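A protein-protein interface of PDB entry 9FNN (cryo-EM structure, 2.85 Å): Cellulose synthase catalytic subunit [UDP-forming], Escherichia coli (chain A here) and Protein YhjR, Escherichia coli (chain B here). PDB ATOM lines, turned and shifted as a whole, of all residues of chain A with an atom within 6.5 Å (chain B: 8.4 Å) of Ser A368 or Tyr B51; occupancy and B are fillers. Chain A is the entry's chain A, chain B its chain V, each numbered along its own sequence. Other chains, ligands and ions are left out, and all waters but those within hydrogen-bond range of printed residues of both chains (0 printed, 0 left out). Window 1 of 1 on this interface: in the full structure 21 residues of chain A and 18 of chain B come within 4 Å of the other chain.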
ATOM      1  N   ILE A 299     -10.063   0.069 -19.917  1.00  0.00           N
ATOM      2  CA  ILE A 299     -10.337  -1.336 -19.645  1.00  0.00           C
ATOM      3  C   ILE A 299      -9.086  -2.159 -19.916  1.00  0.00           C
ATOM      4  O   ILE A 299      -8.413  -1.978 -20.938  1.00  0.00           O
ATOM      5  CB  ILE A 299     -11.524  -1.822 -20.488  1.00  0.00           C
ATOM      6  CG1 ILE A 299     -12.835  -1.276 -19.924  1.00  0.00           C
ATOM      7  CG2 ILE A 299     -11.567  -3.333 -20.541  1.00  0.00           C
ATOM      8  CD1 ILE A 299     -14.062  -1.781 -20.637  1.00  0.00           C
ATOM      9  N   ASP A 300      -8.767  -3.070 -18.996  1.00  0.00           N
ATOM     10  CA  ASP A 300      -7.603  -3.930 -19.155  1.00  0.00           C
ATOM     11  C   ASP A 300      -7.866  -5.012 -20.192  1.00  0.00           C
ATOM     12  O   ASP A 300      -7.965  -6.196 -19.860  1.00  0.00           O
ATOM     13  CB  ASP A 300      -7.206  -4.552 -17.818  1.00  0.00           C
ATOM     14  CG  ASP A 300      -6.588  -3.547 -16.873  1.00  0.00           C
ATOM     15  OD1 ASP A 300      -5.916  -2.612 -17.358  1.00  0.00           O
ATOM     16  OD2 ASP A 300      -6.772  -3.683 -15.648  1.00  0.00           O
ATOM     17  N   PRO A 365     -17.759   1.001 -16.526  1.00  0.00           N
ATOM     18  CA  PRO A 365     -17.161  -0.309 -16.266  1.00  0.00           C
ATOM     19  C   PRO A 365     -15.827  -0.211 -15.551  1.00  0.00           C
ATOM     20  O   PRO A 365     -15.052   0.729 -15.741  1.00  0.00           O
ATOM     21  CB  PRO A 365     -16.980  -0.892 -17.671  1.00  0.00           C
ATOM     22  CG  PRO A 365     -16.823   0.288 -18.534  1.00  0.00           C
ATOM     23  CD  PRO A 365     -17.681   1.368 -17.948  1.00  0.00           C
ATOM     24  N   THR A 366     -15.567  -1.209 -14.714  1.00  0.00           N
ATOM     25  CA  THR A 366     -14.256  -1.363 -14.115  1.00  0.00           C
ATOM     26  C   THR A 366     -13.293  -1.976 -15.124  1.00  0.00           C
ATOM     27  O   THR A 366     -13.694  -2.540 -16.145  1.00  0.00           O
ATOM     28  CB  THR A 366     -14.326  -2.234 -12.863  1.00  0.00           C
ATOM     29  OG1 THR A 366     -14.762  -3.550 -13.221  1.00  0.00           O
ATOM     30  CG2 THR A 366     -15.298  -1.645 -11.861  1.00  0.00           C
ATOM     31  N   ARG A 367     -11.999  -1.859 -14.826  1.00  0.00           N
ATOM     32  CA  ARG A 367     -10.982  -2.339 -15.750  1.00  0.00           C
ATOM     33  C   ARG A 367     -10.924  -3.858 -15.819  1.00  0.00           C
ATOM     34  O   ARG A 367     -10.385  -4.401 -16.787  1.00  0.00           O
ATOM     35  CB  ARG A 367      -9.618  -1.779 -15.357  1.00  0.00           C
ATOM     36  CG  ARG A 367      -9.206  -2.089 -13.932  1.00  0.00           C
ATOM     37  CD  ARG A 367      -8.024  -1.237 -13.520  1.00  0.00           C
ATOM     38  NE  ARG A 367      -7.481  -1.629 -12.227  1.00  0.00           N
ATOM     39  CZ  ARG A 367      -6.422  -2.409 -12.068  1.00  0.00           C
ATOM     40  NH1 ARG A 367      -5.768  -2.904 -13.105  1.00  0.00           N
ATOM     41  NH2 ARG A 367      -6.008  -2.697 -10.839  1.00  0.00           N
ATOM     42  N   SER A 368     -11.469  -4.551 -14.825  1.00  0.00           N
ATOM     43  CA  SER A 368     -11.454  -6.004 -14.783  1.00  0.00           C
ATOM     44  C   SER A 368     -12.671  -6.627 -15.447  1.00  0.00           C
ATOM     45  O   SER A 368     -12.804  -7.853 -15.433  1.00  0.00           O
ATOM     46  CB  SER A 368     -11.366  -6.484 -13.333  1.00  0.00           C
ATOM     47  OG  SER A 368     -10.334  -5.813 -12.634  1.00  0.00           O
ATOM     48  N   PHE A 369     -13.554  -5.813 -16.028  1.00  0.00           N
ATOM     49  CA  PHE A 369     -14.837  -6.308 -16.518  1.00  0.00           C
ATOM     50  C   PHE A 369     -14.653  -7.407 -17.557  1.00  0.00           C
ATOM     51  O   PHE A 369     -15.195  -8.512 -17.420  1.00  0.00           O
ATOM     52  CB  PHE A 369     -15.636  -5.141 -17.094  1.00  0.00           C
ATOM     53  CG  PHE A 369     -16.990  -5.516 -17.608  1.00  0.00           C
ATOM     54  CD1 PHE A 369     -18.062  -5.635 -16.747  1.00  0.00           C
ATOM     55  CD2 PHE A 369     -17.197  -5.727 -18.959  1.00  0.00           C
ATOM     56  CE1 PHE A 369     -19.311  -5.972 -17.219  1.00  0.00           C
ATOM     57  CE2 PHE A 369     -18.444  -6.063 -19.435  1.00  0.00           C
ATOM     58  CZ  PHE A 369     -19.500  -6.185 -18.564  1.00  0.00           C
ATOM     59  N   LEU A 370     -13.862  -7.129 -18.590  1.00  0.00           N
ATOM     60  CA  LEU A 370     -13.704  -8.094 -19.670  1.00  0.00           C
ATOM     61  C   LEU A 370     -12.939  -9.326 -19.204  1.00  0.00           C
ATOM     62  O   LEU A 370     -13.237 -10.442 -19.636  1.00  0.00           O
ATOM     63  CB  LEU A 370     -13.015  -7.438 -20.863  1.00  0.00           C
ATOM     64  CG  LEU A 370     -13.889  -6.672 -21.863  1.00  0.00           C
ATOM     65  CD1 LEU A 370     -14.995  -7.560 -22.390  1.00  0.00           C
ATOM     66  CD2 LEU A 370     -14.464  -5.403 -21.267  1.00  0.00           C
ATOM     67  N   GLN A 371     -11.958  -9.151 -18.319  1.00  0.00           N
ATOM     68  CA  GLN A 371     -11.220 -10.306 -17.819  1.00  0.00           C
ATOM     69  C   GLN A 371     -12.077 -11.175 -16.910  1.00  0.00           C
ATOM     70  O   GLN A 371     -11.906 -12.398 -16.882  1.00  0.00           O
ATOM     71  CB  GLN A 371      -9.959  -9.857 -17.088  1.00  0.00           C
ATOM     72  CG  GLN A 371      -8.886  -9.301 -18.003  1.00  0.00           C
ATOM     73  CD  GLN A 371      -7.528  -9.270 -17.347  1.00  0.00           C
ATOM     74  OE1 GLN A 371      -7.322  -9.867 -16.291  1.00  0.00           O
ATOM     75  NE2 GLN A 371      -6.586  -8.573 -17.969  1.00  0.00           N
ATOM     76  N   MET A 372     -12.992 -10.571 -16.156  1.00  0.00           N
ATOM     77  CA  MET A 372     -13.897 -11.342 -15.317  1.00  0.00           C
ATOM     78  C   MET A 372     -15.062 -11.930 -16.099  1.00  0.00           C
ATOM     79  O   MET A 372     -15.757 -12.807 -15.578  1.00  0.00           O
ATOM     80  CB  MET A 372     -14.432 -10.470 -14.182  1.00  0.00           C
ATOM     81  CG  MET A 372     -13.365  -9.942 -13.246  1.00  0.00           C
ATOM     82  SD  MET A 372     -13.103 -10.987 -11.812  1.00  0.00           S
ATOM     83  CE  MET A 372     -14.711 -10.871 -11.035  1.00  0.00           C
ATOM     84  N   THR A 373     -15.292 -11.474 -17.328  1.00  0.00           N
ATOM     85  CA  THR A 373     -16.438 -11.933 -18.105  1.00  0.00           C
ATOM     86  C   THR A 373     -16.084 -12.920 -19.213  1.00  0.00           C
ATOM     87  O   THR A 373     -16.784 -13.923 -19.380  1.00  0.00           O
ATOM     88  CB  THR A 373     -17.165 -10.730 -18.708  1.00  0.00           C
ATOM     89  OG1 THR A 373     -17.601  -9.861 -17.657  1.00  0.00           O
ATOM     90  CG2 THR A 373     -18.370 -11.178 -19.509  1.00  0.00           C
ATOM     91  N   GLN A 478     -19.267  -4.870 -11.421  1.00  0.00           N
ATOM     92  CA  GLN A 478     -18.160  -4.266 -12.150  1.00  0.00           C
ATOM     93  C   GLN A 478     -18.579  -3.026 -12.926  1.00  0.00           C
ATOM     94  O   GLN A 478     -17.831  -2.573 -13.801  1.00  0.00           O
ATOM     95  CB  GLN A 478     -17.528  -5.292 -13.097  1.00  0.00           C
ATOM     96  CG  GLN A 478     -17.014  -6.547 -12.404  1.00  0.00           C
ATOM     97  CD  GLN A 478     -15.836  -6.278 -11.488  1.00  0.00           C
ATOM     98  OE1 GLN A 478     -16.008  -5.988 -10.305  1.00  0.00           O
ATOM     99  NE2 GLN A 478     -14.630  -6.375 -12.033  1.00  0.00           N
ATOM    100  N   ALA A 791     -13.737   3.737 -11.761  1.00  0.00           N
ATOM    101  CA  ALA A 791     -13.519   2.408 -12.310  1.00  0.00           C
ATOM    102  C   ALA A 791     -12.480   1.637 -11.508  1.00  0.00           C
ATOM    103  O   ALA A 791     -11.517   1.110 -12.074  1.00  0.00           O
ATOM    104  CB  ALA A 791     -13.093   2.501 -13.775  1.00  0.00           C
ATOM    105  N   ALA A 793     -11.996  -1.733  -9.325  1.00  0.00           N
ATOM    106  CA  ALA A 793     -12.673  -3.010  -9.122  1.00  0.00           C
ATOM    107  C   ALA A 793     -12.604  -3.451  -7.664  1.00  0.00           C
ATOM    108  O   ALA A 793     -12.284  -4.594  -7.354  1.00  0.00           O
ATOM    109  CB  ALA A 793     -12.075  -4.067 -10.043  1.00  0.00           C
ATOM    110  N   ASP B  36      -6.730  -3.037  -6.066  1.00  0.00           N
ATOM    111  CA  ASP B  36      -8.146  -3.326  -6.267  1.00  0.00           C
ATOM    112  C   ASP B  36      -8.374  -4.812  -6.515  1.00  0.00           C
ATOM    113  O   ASP B  36      -9.311  -5.406  -5.967  1.00  0.00           O
ATOM    114  CB  ASP B  36      -8.688  -2.503  -7.433  1.00  0.00           C
ATOM    115  CG  ASP B  36      -8.298  -1.042  -7.344  1.00  0.00           C
ATOM    116  OD1 ASP B  36      -8.153  -0.531  -6.215  1.00  0.00           O
ATOM    117  OD2 ASP B  36      -8.134  -0.405  -8.406  1.00  0.00           O
ATOM    118  N   ILE B  37      -7.527  -5.429  -7.340  1.00  0.00           N
ATOM    119  CA  ILE B  37      -7.659  -6.857  -7.606  1.00  0.00           C
ATOM    120  C   ILE B  37      -7.369  -7.662  -6.345  1.00  0.00           C
ATOM    121  O   ILE B  37      -7.996  -8.699  -6.097  1.00  0.00           O
ATOM    122  CB  ILE B  37      -6.748  -7.270  -8.774  1.00  0.00           C
ATOM    123  CG1 ILE B  37      -5.298  -6.865  -8.502  1.00  0.00           C
ATOM    124  CG2 ILE B  37      -7.234  -6.643 -10.069  1.00  0.00           C
ATOM    125  CD1 ILE B  37      -4.336  -7.253  -9.604  1.00  0.00           C
ATOM    126  N   VAL B  38      -6.423  -7.199  -5.525  1.00  0.00           N
ATOM    127  CA  VAL B  38      -6.148  -7.866  -4.256  1.00  0.00           C
ATOM    128  C   VAL B  38      -7.357  -7.768  -3.336  1.00  0.00           C
ATOM    129  O   VAL B  38      -7.709  -8.730  -2.641  1.00  0.00           O
ATOM    130  CB  VAL B  38      -4.887  -7.273  -3.603  1.00  0.00           C
ATOM    131  CG1 VAL B  38      -4.571  -7.996  -2.302  1.00  0.00           C
ATOM    132  CG2 VAL B  38      -3.708  -7.349  -4.561  1.00  0.00           C
ATOM    133  N   LEU B  40     -10.477  -7.504  -4.306  1.00  0.00           N
ATOM    134  CA  LEU B  40     -11.471  -8.432  -4.838  1.00  0.00           C
ATOM    135  C   LEU B  40     -11.153  -9.869  -4.450  1.00  0.00           C
ATOM    136  O   LEU B  40     -12.050 -10.629  -4.065  1.00  0.00           O
ATOM    137  CB  LEU B  40     -11.558  -8.299  -6.356  1.00  0.00           C
ATOM    138  CG  LEU B  40     -12.805  -7.601  -6.891  1.00  0.00           C
ATOM    139  CD1 LEU B  40     -12.865  -7.699  -8.405  1.00  0.00           C
ATOM    140  CD2 LEU B  40     -14.058  -8.181  -6.257  1.00  0.00           C
ATOM    141  N   LYS B  41      -9.881 -10.263  -4.548  1.00  0.00           N
ATOM    142  CA  LYS B  41      -9.499 -11.625  -4.189  1.00  0.00           C
ATOM    143  C   LYS B  41      -9.747 -11.896  -2.711  1.00  0.00           C
ATOM    144  O   LYS B  41     -10.213 -12.980  -2.340  1.00  0.00           O
ATOM    145  CB  LYS B  41      -8.033 -11.873  -4.545  1.00  0.00           C
ATOM    146  CG  LYS B  41      -7.760 -11.921  -6.039  1.00  0.00           C
ATOM    147  CD  LYS B  41      -6.293 -12.193  -6.325  1.00  0.00           C
ATOM    148  CE  LYS B  41      -6.026 -12.261  -7.820  1.00  0.00           C
ATOM    149  NZ  LYS B  41      -4.588 -12.510  -8.114  1.00  0.00           N
ATOM    150  N   LEU B  46     -11.884 -16.124  -5.866  1.00  0.00           N
ATOM    151  CA  LEU B  46     -11.043 -15.813  -7.016  1.00  0.00           C
ATOM    152  C   LEU B  46      -9.555 -16.044  -6.736  1.00  0.00           C
ATOM    153  O   LEU B  46      -8.764 -15.095  -6.727  1.00  0.00           O
ATOM    154  CB  LEU B  46     -11.285 -14.383  -7.480  1.00  0.00           C
ATOM    155  CG  LEU B  46     -12.386 -14.122  -8.509  1.00  0.00           C
ATOM    156  CD1 LEU B  46     -13.717 -14.744  -8.109  1.00  0.00           C
ATOM    157  CD2 LEU B  46     -12.537 -12.627  -8.709  1.00  0.00           C
ATOM    158  N   ASP B  48      -7.531 -18.276  -8.565  1.00  0.00           N
ATOM    159  CA  ASP B  48      -6.825 -18.789  -9.726  1.00  0.00           C
ATOM    160  C   ASP B  48      -6.938 -17.890 -10.947  1.00  0.00           C
ATOM    161  O   ASP B  48      -6.404 -18.241 -12.006  1.00  0.00           O
ATOM    162  CB  ASP B  48      -7.334 -20.194 -10.080  1.00  0.00           C
ATOM    163  CG  ASP B  48      -7.153 -21.182  -8.944  1.00  0.00           C
ATOM    164  OD1 ASP B  48      -6.174 -21.042  -8.181  1.00  0.00           O
ATOM    165  OD2 ASP B  48      -7.992 -22.099  -8.812  1.00  0.00           O
ATOM    166  N   ILE B  49      -7.611 -16.748 -10.840  1.00  0.00           N
ATOM    167  CA  ILE B  49      -7.749 -15.823 -11.958  1.00  0.00           C
ATOM    168  C   ILE B  49      -6.543 -14.892 -11.913  1.00  0.00           C
ATOM    169  O   ILE B  49      -6.493 -13.953 -11.117  1.00  0.00           O
ATOM    170  CB  ILE B  49      -9.070 -15.052 -11.906  1.00  0.00           C
ATOM    171  CG1 ILE B  49     -10.259 -15.997 -12.106  1.00  0.00           C
ATOM    172  CG2 ILE B  49      -9.094 -13.964 -12.964  1.00  0.00           C
ATOM    173  CD1 ILE B  49     -10.800 -16.602 -10.826  1.00  0.00           C
ATOM    174  N   ASP B  50      -5.556 -15.161 -12.766  1.00  0.00           N
ATOM    175  CA  ASP B  50      -4.363 -14.326 -12.843  1.00  0.00           C
ATOM    176  C   ASP B  50      -4.678 -13.077 -13.657  1.00  0.00           C
ATOM    177  O   ASP B  50      -5.100 -13.171 -14.814  1.00  0.00           O
ATOM    178  CB  ASP B  50      -3.203 -15.104 -13.459  1.00  0.00           C
ATOM    179  CG  ASP B  50      -3.617 -15.904 -14.678  1.00  0.00           C
ATOM    180  OD1 ASP B  50      -4.832 -15.977 -14.959  1.00  0.00           O
ATOM    181  OD2 ASP B  50      -2.728 -16.462 -15.355  1.00  0.00           O
ATOM    182  N   TYR B  51      -4.468 -11.911 -13.058  1.00  0.00           N
ATOM    183  CA  TYR B  51      -4.870 -10.652 -13.665  1.00  0.00           C
ATOM    184  C   TYR B  51      -3.791 -10.160 -14.619  1.00  0.00           C
ATOM    185  O   TYR B  51      -2.626 -10.024 -14.234  1.00  0.00           O
ATOM    186  CB  TYR B  51      -5.146  -9.606 -12.588  1.00  0.00           C
ATOM    187  CG  TYR B  51      -5.900  -8.405 -13.094  1.00  0.00           C
ATOM    188  CD1 TYR B  51      -7.246  -8.496 -13.409  1.00  0.00           C
ATOM    189  CD2 TYR B  51      -5.270  -7.181 -13.255  1.00  0.00           C
ATOM    190  CE1 TYR B  51      -7.944  -7.406 -13.871  1.00  0.00           C
ATOM    191  CE2 TYR B  51      -5.963  -6.082 -13.717  1.00  0.00           C
ATOM    192  CZ  TYR B  51      -7.300  -6.202 -14.023  1.00  0.00           C
ATOM    193  OH  TYR B  51      -8.000  -5.112 -14.485  1.00  0.00           O
ATOM    194  N   ALA B  52      -4.185  -9.888 -15.861  1.00  0.00           N
ATOM    195  CA  ALA B  52      -3.277  -9.400 -16.893  1.00  0.00           C
ATOM    196  C   ALA B  52      -3.516  -7.904 -17.062  1.00  0.00           C
ATOM    197  O   ALA B  52      -4.465  -7.488 -17.729  1.00  0.00           O
ATOM    198  CB  ALA B  52      -3.491 -10.153 -18.201  1.00  0.00           C
ATOM    199  N   ASP B  53      -2.649  -7.096 -16.457  1.00  0.00           N
ATOM    200  CA  ASP B  53      -2.779  -5.641 -16.506  1.00  0.00           C
ATOM    201  C   ASP B  53      -2.200  -5.159 -17.828  1.00  0.00           C
ATOM    202  O   ASP B  53      -1.015  -4.846 -17.938  1.00  0.00           O
ATOM    203  CB  ASP B  53      -2.081  -4.999 -15.316  1.00  0.00           C
ATOM    204  CG  ASP B  53      -2.606  -3.611 -15.012  1.00  0.00           C
ATOM    205  OD1 ASP B  53      -3.064  -2.925 -15.950  1.00  0.00           O
ATOM    206  OD2 ASP B  53      -2.562  -3.203 -13.833  1.00  0.00           O
ATOM    207  N   ILE B  54      -3.055  -5.099 -18.852  1.00  0.00           N
ATOM    208  CA  ILE B  54      -2.576  -4.760 -20.187  1.00  0.00           C
ATOM    209  C   ILE B  54      -2.221  -3.282 -20.282  1.00  0.00           C
ATOM    210  O   ILE B  54      -1.392  -2.891 -21.114  1.00  0.00           O
ATOM    211  CB  ILE B  54      -3.613  -5.166 -21.251  1.00  0.00           C
ATOM    212  CG1 ILE B  54      -2.943  -5.314 -22.616  1.00  0.00           C
ATOM    213  CG2 ILE B  54      -4.716  -4.136 -21.341  1.00  0.00           C
ATOM    214  CD1 ILE B  54      -1.819  -6.328 -22.640  1.00  0.00           C
ATOM    215  N   SER B  55      -2.826  -2.439 -19.443  1.00  0.00           N
ATOM    216  CA  SER B  55      -2.477  -1.021 -19.451  1.00  0.00           C
ATOM    217  C   SER B  55      -1.036  -0.806 -19.009  1.00  0.00           C
ATOM    218  O   SER B  55      -0.300  -0.027 -19.627  1.00  0.00           O
ATOM    219  CB  SER B  55      -3.438  -0.240 -18.558  1.00  0.00           C
ATOM    220  OG  SER B  55      -3.112   1.138 -18.541  1.00  0.00           O
ATOM    221  N   GLN B  56      -0.611  -1.498 -17.948  1.00  0.00           N
ATOM    222  CA  GLN B  56       0.772  -1.393 -17.500  1.00  0.00           C
ATOM    223  C   GLN B  56       1.734  -1.900 -18.564  1.00  0.00           C
ATOM    224  O   GLN B  56       2.785  -1.294 -18.798  1.00  0.00           O
ATOM    225  CB  GLN B  56       0.967  -2.167 -16.198  1.00  0.00           C
ATOM    226  CG  GLN B  56       0.155  -1.640 -15.030  1.00  0.00           C
ATOM    227  CD  GLN B  56       0.564  -0.244 -14.615  1.00  0.00           C
ATOM    228  OE1 GLN B  56      -0.266   0.557 -14.186  1.00  0.00           O
ATOM    229  NE2 GLN B  56       1.853   0.055 -14.731  1.00  0.00           N
ATOM    230  N   ARG B  57       1.393  -3.011 -19.218  1.00  0.00           N
ATOM    231  CA  ARG B  57       2.258  -3.544 -20.264  1.00  0.00           C
ATOM    232  C   ARG B  57       2.376  -2.577 -21.434  1.00  0.00           C
ATOM    233  O   ARG B  57       3.471  -2.379 -21.975  1.00  0.00           O
ATOM    234  CB  ARG B  57       1.737  -4.897 -20.741  1.00  0.00           C
ATOM    235  CG  ARG B  57       2.000  -6.035 -19.777  1.00  0.00           C
ATOM    236  CD  ARG B  57       2.011  -7.369 -20.506  1.00  0.00           C
ATOM    237  NE  ARG B  57       0.822  -8.166 -20.227  1.00  0.00           N
ATOM    238  CZ  ARG B  57       0.747  -9.077 -19.267  1.00  0.00           C
ATOM    239  NH1 ARG B  57       1.771  -9.324 -18.466  1.00  0.00           N
ATOM    240  NH2 ARG B  57      -0.383  -9.759 -19.109  1.00  0.00           N
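The side-chain carboxylate (OD2) of Asp A300 lies close to the side-chain hydroxyl (OH) of Tyr B51, 2.2 Å away.
The side-chain carboxylate of Asp A300 lies close to the side-chain carboxylate of Asp B53, 3.2 Å away.
O of Arg A367 lies close to OH of Tyr B51, 3.4 Å away.
O of Ala A793 lies close to O of Asp B36.
NH1 of Arg A367 lies within salt-bridge range of OD2 of Asp B53 (3.3 Å).
OE1 of Gln A371 is in hydrogen-bond range of N of Ala B52.
NH2 of Arg A367 is in salt-bridge range of OD2 of Asp B36.
The side-chain hydroxyl (OG) of Ser A368 is in hydrogen-bond range of the side-chain hydroxyl (OH) of Tyr B51 (3.1 Å).
N of Gln B56 lies within hydrogen-bond range of OD1 of Asp B53 (3.5 Å).
The side-chain amide nitrogen of Gln A371 is in hydrogen-bond range of the backbone carbonyl oxygen of Asp A300 (3.3 Å).
The side-chain carboxylate (OD2) of Asp A300 lies within salt-bridge range of the guanidinium group (NH1) of Arg A367 (2.8 Å).
CG2 of Ile B54 touches C of Asp A300, 3.5 Å away.
Asp A300 touches Ser B55.
Tyr B51 touches Gln A371.
SD of Met A372 touches CD2 of Leu B46, at 3.6 Å.
CG of Leu B40 touches O of Ala A793 (3.1 Å).
Of chain A, only Asp A300, Arg A367, Ser A368 and Gln A371 come within 4 Å of Tyr B51.
Of the printed residues of chain A, Leu B46 touches Met A372 (3.6 Å).
Of the printed residues of chain A, Ala B52 touches Gln A371.
Printed residues of chain B within 4 Å of Ala A793: Asp B36 and Leu B40.
Lys B41 touches none of the printed residues of chain A.
Arg B57 touches none of the printed residues of chain A.
The nearest printed residue of chain B that does not touch Asp A300 is Ala B52 (4.02 Å).
Of the 14 printed residues of chain A, 6 touch a printed residue of chain B.
Hydrophobic or aromatic side chains of chain A that line the printed part of chain B: Met A372.
Of the 16 printed residues of chain B, 8 touch a printed residue of chain A.
Hydrophobic or aromatic side chains of chain B within 4 Å of the printed part of chain A: Leu B40, Leu B46, Tyr B51, Ala B52 and Ile B54.
Along chain B the printed residues that touch a printed residue of chain A span positions 36 to 55.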
